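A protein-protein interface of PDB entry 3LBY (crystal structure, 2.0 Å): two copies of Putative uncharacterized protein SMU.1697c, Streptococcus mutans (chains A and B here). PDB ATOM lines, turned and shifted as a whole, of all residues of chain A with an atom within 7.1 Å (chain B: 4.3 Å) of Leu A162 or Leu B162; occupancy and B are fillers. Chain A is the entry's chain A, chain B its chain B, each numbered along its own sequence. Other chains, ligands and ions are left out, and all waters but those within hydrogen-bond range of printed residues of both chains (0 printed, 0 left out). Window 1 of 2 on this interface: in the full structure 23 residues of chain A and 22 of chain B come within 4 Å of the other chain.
The backbone carbonyl oxygen of Val A160 lies within hydrogen-bond range of the backbone NH of Leu B166, at 2.8 Å.
The backbone NH of Leu A162 lies within hydrogen-bond range of the backbone carbonyl oxygen of Gln B164 (2.7 Å).
The backbone carbonyl oxygen (O) of Gln A164 sits at hydrogen-bond distance from the backbone NH (N) of Leu B162, 2.7 Å away.
O of Leu A162 sits close to O of Leu B162 (3.4 Å).
N of Pro A165 lies close to SD of Met B161, 3.7 Å away.
The backbone carbonyl oxygen of Met A161 is in hydrogen-bond range of the backbone NH of Met A177 (2.9 Å).
The backbone NH (N) of Tyr A163 is in hydrogen-bond range of the backbone carbonyl oxygen (O) of Leu A175, at 2.9 Å.
O of Leu B175 lies within hydrogen-bond range of N of Tyr B163.
Among the printed residues, merely in contact across the chains: Met A161 with Tyr B163 (3.6 Å), Met A161 with Gln B164 (3.3 Å), Leu A162 with Tyr B163 (3.3 Å), Leu A162 with Leu B166 (3.8 Å), Tyr A163 with Met B161 (3.5 Å), Tyr A163 with Leu B162 (3.3 Å), Tyr A163 with Tyr B163 (3.97 Å), Gln A164 with Met B161 (3.4 Å), Leu A166 with Leu B162 (3.8 Å) and Met A177 with Tyr B163 (3.7 Å).
Leu A162 touches just these residues of chain B: Leu B162, Tyr B163, Gln B164 and Leu B166.
Of the printed residues of chain B, Tyr A163 touches Met B161, Leu B162 and Tyr B163.
Of the printed residues of chain B, Pro A165 touches Met B161 (3.4 Å).
Val A176 touches none of the printed residues of chain B.
Of the printed residues of chain A, Leu B162 touches Leu A162 (3.4 Å), Tyr A163 (3.3 Å), Gln A164 (2.7 Å) and Leu A166 (3.8 Å).
Of the printed residues of chain A, Tyr B163 touches Met A161 (3.6 Å), Leu A162 (3.3 Å), Tyr A163 (3.97 Å) and Met A177 (3.7 Å).
The nearest residue of chain A that does not touch Leu B162 is Pro A165 (4.8 Å).
The nearest printed residue of chain A that does not touch Met B161 is Leu A166 (4.5 Å).
Printed residues of chain B that touch a printed residue of chain A: Met B161, Leu B162, Tyr B163, Gln B164 and Leu B166.
Hydrophobic or aromatic side chains of chain B that line the printed part of chain A: Met B161, Leu B162, Tyr B163 and Leu B166.
Along chain B the printed residues that touch a printed residue of chain A span positions 161 to 166.
Among the printed residues, no Asp or Glu carboxylate lies within 4 Å of a Lys or Arg side-chain nitrogen of the other chain.
Met A161 touches Gln B164, and with the chains exchanged Gln A164 touches Met B161.
Leu A162 touches Gln B164, and with the chains exchanged Gln A164 touches Leu B162.
Leu A162 touches Leu B166, and with the chains exchanged Leu A166 touches Leu B162.
Tyr A163 touches its own counterpart, Tyr B163.
Positions printed for both chains: 161, 162, 163, 164, 166, 174 and 175.
Of the 15 pairs that touch across the chains among the printed residues, 12 have their exchanged pair printed and touching as well.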
ATOM      1  N   VAL A 132      19.994  26.312  27.192  1.00  0.00           N
ATOM      2  CA  VAL A 132      18.917  25.716  27.973  1.00  0.00           C
ATOM      3  C   VAL A 132      19.388  25.384  29.389  1.00  0.00           C
ATOM      4  O   VAL A 132      20.233  24.516  29.566  1.00  0.00           O
ATOM      5  CB  VAL A 132      18.414  24.431  27.302  1.00  0.00           C
ATOM      6  CG1 VAL A 132      17.338  23.769  28.148  1.00  0.00           C
ATOM      7  CG2 VAL A 132      17.896  24.741  25.895  1.00  0.00           C
ATOM      8  N   LEU A 147      13.345  21.092  22.772  1.00  0.00           N
ATOM      9  CA  LEU A 147      13.904  19.976  22.029  1.00  0.00           C
ATOM     10  C   LEU A 147      12.870  19.446  21.032  1.00  0.00           C
ATOM     11  O   LEU A 147      13.199  19.173  19.877  1.00  0.00           O
ATOM     12  CB  LEU A 147      14.371  18.867  22.978  1.00  0.00           C
ATOM     13  CG  LEU A 147      15.611  19.211  23.818  1.00  0.00           C
ATOM     14  CD1 LEU A 147      15.929  18.114  24.836  1.00  0.00           C
ATOM     15  CD2 LEU A 147      16.813  19.463  22.916  1.00  0.00           C
ATOM     16  N   VAL A 160      19.873  21.919  12.737  1.00  0.00           N
ATOM     17  CA  VAL A 160      19.777  22.022  14.197  1.00  0.00           C
ATOM     18  C   VAL A 160      20.754  21.065  14.870  1.00  0.00           C
ATOM     19  O   VAL A 160      20.692  19.854  14.640  1.00  0.00           O
ATOM     20  CB  VAL A 160      18.363  21.692  14.703  1.00  0.00           C
ATOM     21  CG1 VAL A 160      18.286  21.878  16.218  1.00  0.00           C
ATOM     22  CG2 VAL A 160      17.318  22.572  14.002  1.00  0.00           C
ATOM     23  N   MET A 161      21.643  21.612  15.701  1.00  0.00           N
ATOM     24  CA  MET A 161      22.653  20.811  16.386  1.00  0.00           C
ATOM     25  C   MET A 161      22.523  20.945  17.895  1.00  0.00           C
ATOM     26  O   MET A 161      22.312  22.047  18.407  1.00  0.00           O
ATOM     27  CB  MET A 161      24.069  21.247  15.980  1.00  0.00           C
ATOM     28  CG  MET A 161      24.386  21.129  14.496  1.00  0.00           C
ATOM     29  SD  MET A 161      24.422  19.435  13.863  1.00  0.00           S
ATOM     30  CE  MET A 161      25.227  18.581  15.170  1.00  0.00           C
ATOM     31  N   LEU A 162      22.665  19.821  18.595  1.00  0.00           N
ATOM     32  CA  LEU A 162      22.746  19.809  20.056  1.00  0.00           C
ATOM     33  C   LEU A 162      24.211  19.783  20.496  1.00  0.00           C
ATOM     34  O   LEU A 162      25.008  19.034  19.932  1.00  0.00           O
ATOM     35  CB  LEU A 162      22.036  18.568  20.597  1.00  0.00           C
ATOM     36  CG  LEU A 162      22.091  18.312  22.103  1.00  0.00           C
ATOM     37  CD1 LEU A 162      21.321  19.391  22.865  1.00  0.00           C
ATOM     38  CD2 LEU A 162      21.544  16.931  22.438  1.00  0.00           C
ATOM     39  N   TYR A 163      24.558  20.604  21.486  1.00  0.00           N
ATOM     40  CA  TYR A 163      25.890  20.595  22.097  1.00  0.00           C
ATOM     41  C   TYR A 163      25.743  20.522  23.620  1.00  0.00           C
ATOM     42  O   TYR A 163      25.405  21.518  24.293  1.00  0.00           O
ATOM     43  CB  TYR A 163      26.696  21.827  21.673  1.00  0.00           C
ATOM     44  CG  TYR A 163      28.160  21.819  22.096  1.00  0.00           C
ATOM     45  CD1 TYR A 163      29.059  20.903  21.568  1.00  0.00           C
ATOM     46  CD2 TYR A 163      28.637  22.742  23.027  1.00  0.00           C
ATOM     47  CE1 TYR A 163      30.395  20.902  21.953  1.00  0.00           C
ATOM     48  CE2 TYR A 163      29.964  22.751  23.419  1.00  0.00           C
ATOM     49  CZ  TYR A 163      30.845  21.833  22.882  1.00  0.00           C
ATOM     50  OH  TYR A 163      32.170  21.852  23.272  1.00  0.00           O
ATOM     51  N   GLN A 164      25.990  19.326  24.152  1.00  0.00           N
ATOM     52  CA  GLN A 164      25.605  18.982  25.517  1.00  0.00           C
ATOM     53  C   GLN A 164      26.671  18.167  26.259  1.00  0.00           C
ATOM     54  O   GLN A 164      27.153  17.161  25.750  1.00  0.00           O
ATOM     55  CB  GLN A 164      24.311  18.166  25.483  1.00  0.00           C
ATOM     56  CG  GLN A 164      23.713  17.917  26.860  1.00  0.00           C
ATOM     57  CD  GLN A 164      22.413  17.146  26.798  1.00  0.00           C
ATOM     58  OE1 GLN A 164      22.242  16.268  25.959  1.00  0.00           O
ATOM     59  NE2 GLN A 164      21.491  17.464  27.698  1.00  0.00           N
ATOM     60  N   PRO A 165      27.007  18.581  27.488  1.00  0.00           N
ATOM     61  CA  PRO A 165      27.939  17.829  28.339  1.00  0.00           C
ATOM     62  C   PRO A 165      27.348  16.476  28.728  1.00  0.00           C
ATOM     63  O   PRO A 165      26.167  16.416  29.062  1.00  0.00           O
ATOM     64  CB  PRO A 165      28.065  18.710  29.599  1.00  0.00           C
ATOM     65  CG  PRO A 165      27.508  20.052  29.218  1.00  0.00           C
ATOM     66  CD  PRO A 165      26.471  19.780  28.163  1.00  0.00           C
ATOM     67  N   LEU A 166      28.145  15.409  28.698  1.00  0.00           N
ATOM     68  CA  LEU A 166      27.630  14.079  29.017  1.00  0.00           C
ATOM     69  C   LEU A 166      28.029  13.546  30.406  1.00  0.00           C
ATOM     70  O   LEU A 166      27.332  12.705  30.966  1.00  0.00           O
ATOM     71  CB  LEU A 166      28.052  13.064  27.955  1.00  0.00           C
ATOM     72  CG  LEU A 166      27.338  13.095  26.597  1.00  0.00           C
ATOM     73  CD1 LEU A 166      27.857  11.968  25.726  1.00  0.00           C
ATOM     74  CD2 LEU A 166      25.829  12.979  26.775  1.00  0.00           C
ATOM     75  N   PHE A 174      22.898  23.323  28.354  1.00  0.00           N
ATOM     76  CA  PHE A 174      23.391  22.907  27.053  1.00  0.00           C
ATOM     77  C   PHE A 174      22.942  23.864  25.962  1.00  0.00           C
ATOM     78  O   PHE A 174      22.073  24.720  26.184  1.00  0.00           O
ATOM     79  CB  PHE A 174      22.965  21.470  26.740  1.00  0.00           C
ATOM     80  CG  PHE A 174      21.480  21.278  26.612  1.00  0.00           C
ATOM     81  CD1 PHE A 174      20.825  21.577  25.428  1.00  0.00           C
ATOM     82  CD2 PHE A 174      20.740  20.769  27.668  1.00  0.00           C
ATOM     83  CE1 PHE A 174      19.456  21.385  25.302  1.00  0.00           C
ATOM     84  CE2 PHE A 174      19.372  20.577  27.551  1.00  0.00           C
ATOM     85  CZ  PHE A 174      18.727  20.886  26.365  1.00  0.00           C
ATOM     86  N   LEU A 175      23.536  23.703  24.784  1.00  0.00           N
ATOM     87  CA  LEU A 175      23.327  24.628  23.682  1.00  0.00           C
ATOM     88  C   LEU A 175      22.573  23.970  22.530  1.00  0.00           C
ATOM     89  O   LEU A 175      22.901  22.856  22.120  1.00  0.00           O
ATOM     90  CB  LEU A 175      24.676  25.159  23.184  1.00  0.00           C
ATOM     91  CG  LEU A 175      24.701  26.043  21.926  1.00  0.00           C
ATOM     92  CD1 LEU A 175      23.931  27.353  22.155  1.00  0.00           C
ATOM     93  CD2 LEU A 175      26.139  26.340  21.500  1.00  0.00           C
ATOM     94  N   VAL A 176      21.561  24.660  22.015  1.00  0.00           N
ATOM     95  CA  VAL A 176      20.957  24.279  20.728  1.00  0.00           C
ATOM     96  C   VAL A 176      21.337  25.350  19.732  1.00  0.00           C
ATOM     97  O   VAL A 176      21.067  26.536  19.959  1.00  0.00           O
ATOM     98  CB  VAL A 176      19.425  24.162  20.815  1.00  0.00           C
ATOM     99  CG1 VAL A 176      18.807  23.872  19.434  1.00  0.00           C
ATOM    100  CG2 VAL A 176      19.040  23.071  21.796  1.00  0.00           C
ATOM    101  N   MET A 177      21.998  24.930  18.651  1.00  0.00           N
ATOM    102  CA  MET A 177      22.425  25.821  17.576  1.00  0.00           C
ATOM    103  C   MET A 177      21.486  25.655  16.389  1.00  0.00           C
ATOM    104  O   MET A 177      21.193  24.528  15.988  1.00  0.00           O
ATOM    105  CB  MET A 177      23.852  25.473  17.120  1.00  0.00           C
ATOM    106  CG  MET A 177      24.969  25.849  18.130  1.00  0.00           C
ATOM    107  SD  MET A 177      26.486  24.906  17.857  1.00  0.00           S
ATOM    108  CE  MET A 177      25.967  23.343  18.484  1.00  0.00           C
ATOM    109  N   MET B 161      31.663  15.734  25.666  1.00  0.00           N
ATOM    110  CA  MET B 161      30.603  16.527  25.039  1.00  0.00           C
ATOM    111  C   MET B 161      29.933  15.737  23.921  1.00  0.00           C
ATOM    112  O   MET B 161      30.593  14.989  23.193  1.00  0.00           O
ATOM    113  CB  MET B 161      31.160  17.831  24.461  1.00  0.00           C
ATOM    114  CG  MET B 161      31.768  18.767  25.483  1.00  0.00           C
ATOM    115  SD  MET B 161      30.543  19.368  26.671  1.00  0.00           S
ATOM    116  CE  MET B 161      29.372  20.103  25.597  1.00  0.00           C
ATOM    117  N   LEU B 162      28.620  15.915  23.806  1.00  0.00           N
ATOM    118  CA  LEU B 162      27.828  15.338  22.731  1.00  0.00           C
ATOM    119  C   LEU B 162      27.578  16.433  21.690  1.00  0.00           C
ATOM    120  O   LEU B 162      27.257  17.574  22.046  1.00  0.00           O
ATOM    121  CB  LEU B 162      26.492  14.811  23.274  1.00  0.00           C
ATOM    122  CG  LEU B 162      25.458  14.359  22.222  1.00  0.00           C
ATOM    123  CD1 LEU B 162      25.962  13.129  21.499  1.00  0.00           C
ATOM    124  CD2 LEU B 162      24.096  14.085  22.862  1.00  0.00           C
ATOM    125  N   TYR B 163      27.757  16.092  20.416  1.00  0.00           N
ATOM    126  CA  TYR B 163      27.479  17.010  19.304  1.00  0.00           C
ATOM    127  C   TYR B 163      26.623  16.223  18.313  1.00  0.00           C
ATOM    128  O   TYR B 163      27.118  15.328  17.599  1.00  0.00           O
ATOM    129  CB  TYR B 163      28.782  17.478  18.650  1.00  0.00           C
ATOM    130  CG  TYR B 163      28.635  18.516  17.542  1.00  0.00           C
ATOM    131  CD1 TYR B 163      28.250  19.818  17.834  1.00  0.00           C
ATOM    132  CD2 TYR B 163      28.921  18.202  16.214  1.00  0.00           C
ATOM    133  CE1 TYR B 163      28.130  20.772  16.850  1.00  0.00           C
ATOM    134  CE2 TYR B 163      28.798  19.163  15.201  1.00  0.00           C
ATOM    135  CZ  TYR B 163      28.402  20.442  15.537  1.00  0.00           C
ATOM    136  OH  TYR B 163      28.285  21.414  14.589  1.00  0.00           O
ATOM    137  N   GLN B 164      25.335  16.548  18.284  1.00  0.00           N
ATOM    138  CA  GLN B 164      24.359  15.699  17.618  1.00  0.00           C
ATOM    139  C   GLN B 164      23.306  16.490  16.844  1.00  0.00           C
ATOM    140  O   GLN B 164      22.686  17.390  17.400  1.00  0.00           O
ATOM    141  CB  GLN B 164      23.660  14.859  18.668  1.00  0.00           C
ATOM    142  CG  GLN B 164      22.742  13.814  18.112  1.00  0.00           C
ATOM    143  CD  GLN B 164      22.068  13.037  19.210  1.00  0.00           C
ATOM    144  OE1 GLN B 164      21.475  13.619  20.116  1.00  0.00           O
ATOM    145  NE2 GLN B 164      22.162  11.714  19.144  1.00  0.00           N
ATOM    146  N   LEU B 166      19.758  17.325  15.408  1.00  0.00           N
ATOM    147  CA  LEU B 166      18.469  17.050  16.024  1.00  0.00           C
ATOM    148  C   LEU B 166      17.328  16.925  15.018  1.00  0.00           C
ATOM    149  O   LEU B 166      16.321  16.290  15.317  1.00  0.00           O
ATOM    150  CB  LEU B 166      18.116  18.143  17.041  1.00  0.00           C
ATOM    151  CG  LEU B 166      19.026  18.228  18.269  1.00  0.00           C
ATOM    152  CD1 LEU B 166      18.567  19.356  19.208  1.00  0.00           C
ATOM    153  CD2 LEU B 166      19.065  16.885  18.990  1.00  0.00           C
ATOM    154  N   PHE B 174      26.478  10.806  15.040  1.00  0.00           N
ATOM    155  CA  PHE B 174      26.751  11.896  15.970  1.00  0.00           C
ATOM    156  C   PHE B 174      28.128  11.724  16.597  1.00  0.00           C
ATOM    157  O   PHE B 174      28.745  10.666  16.474  1.00  0.00           O
ATOM    158  CB  PHE B 174      25.642  12.031  17.017  1.00  0.00           C
ATOM    159  CG  PHE B 174      25.552  10.875  17.966  1.00  0.00           C
ATOM    160  CD1 PHE B 174      26.351  10.826  19.095  1.00  0.00           C
ATOM    161  CD2 PHE B 174      24.649   9.846  17.744  1.00  0.00           C
ATOM    162  CE1 PHE B 174      26.264   9.769  19.981  1.00  0.00           C
ATOM    163  CE2 PHE B 174      24.557   8.783  18.623  1.00  0.00           C
ATOM    164  CZ  PHE B 174      25.365   8.741  19.742  1.00  0.00           C
ATOM    165  N   LEU B 175      28.606  12.772  17.256  1.00  0.00           N
ATOM    166  CA  LEU B 175      29.973  12.810  17.745  1.00  0.00           C
ATOM    167  C   LEU B 175      30.011  12.950  19.257  1.00  0.00           C
ATOM    168  O   LEU B 175      29.286  13.771  19.830  1.00  0.00           O
ATOM    169  CB  LEU B 175      30.713  13.993  17.110  1.00  0.00           C
ATOM    170  CG  LEU B 175      32.108  14.310  17.659  1.00  0.00           C
ATOM    171  CD1 LEU B 175      33.069  13.167  17.338  1.00  0.00           C
ATOM    172  CD2 LEU B 175      32.635  15.625  17.084  1.00  0.00           C
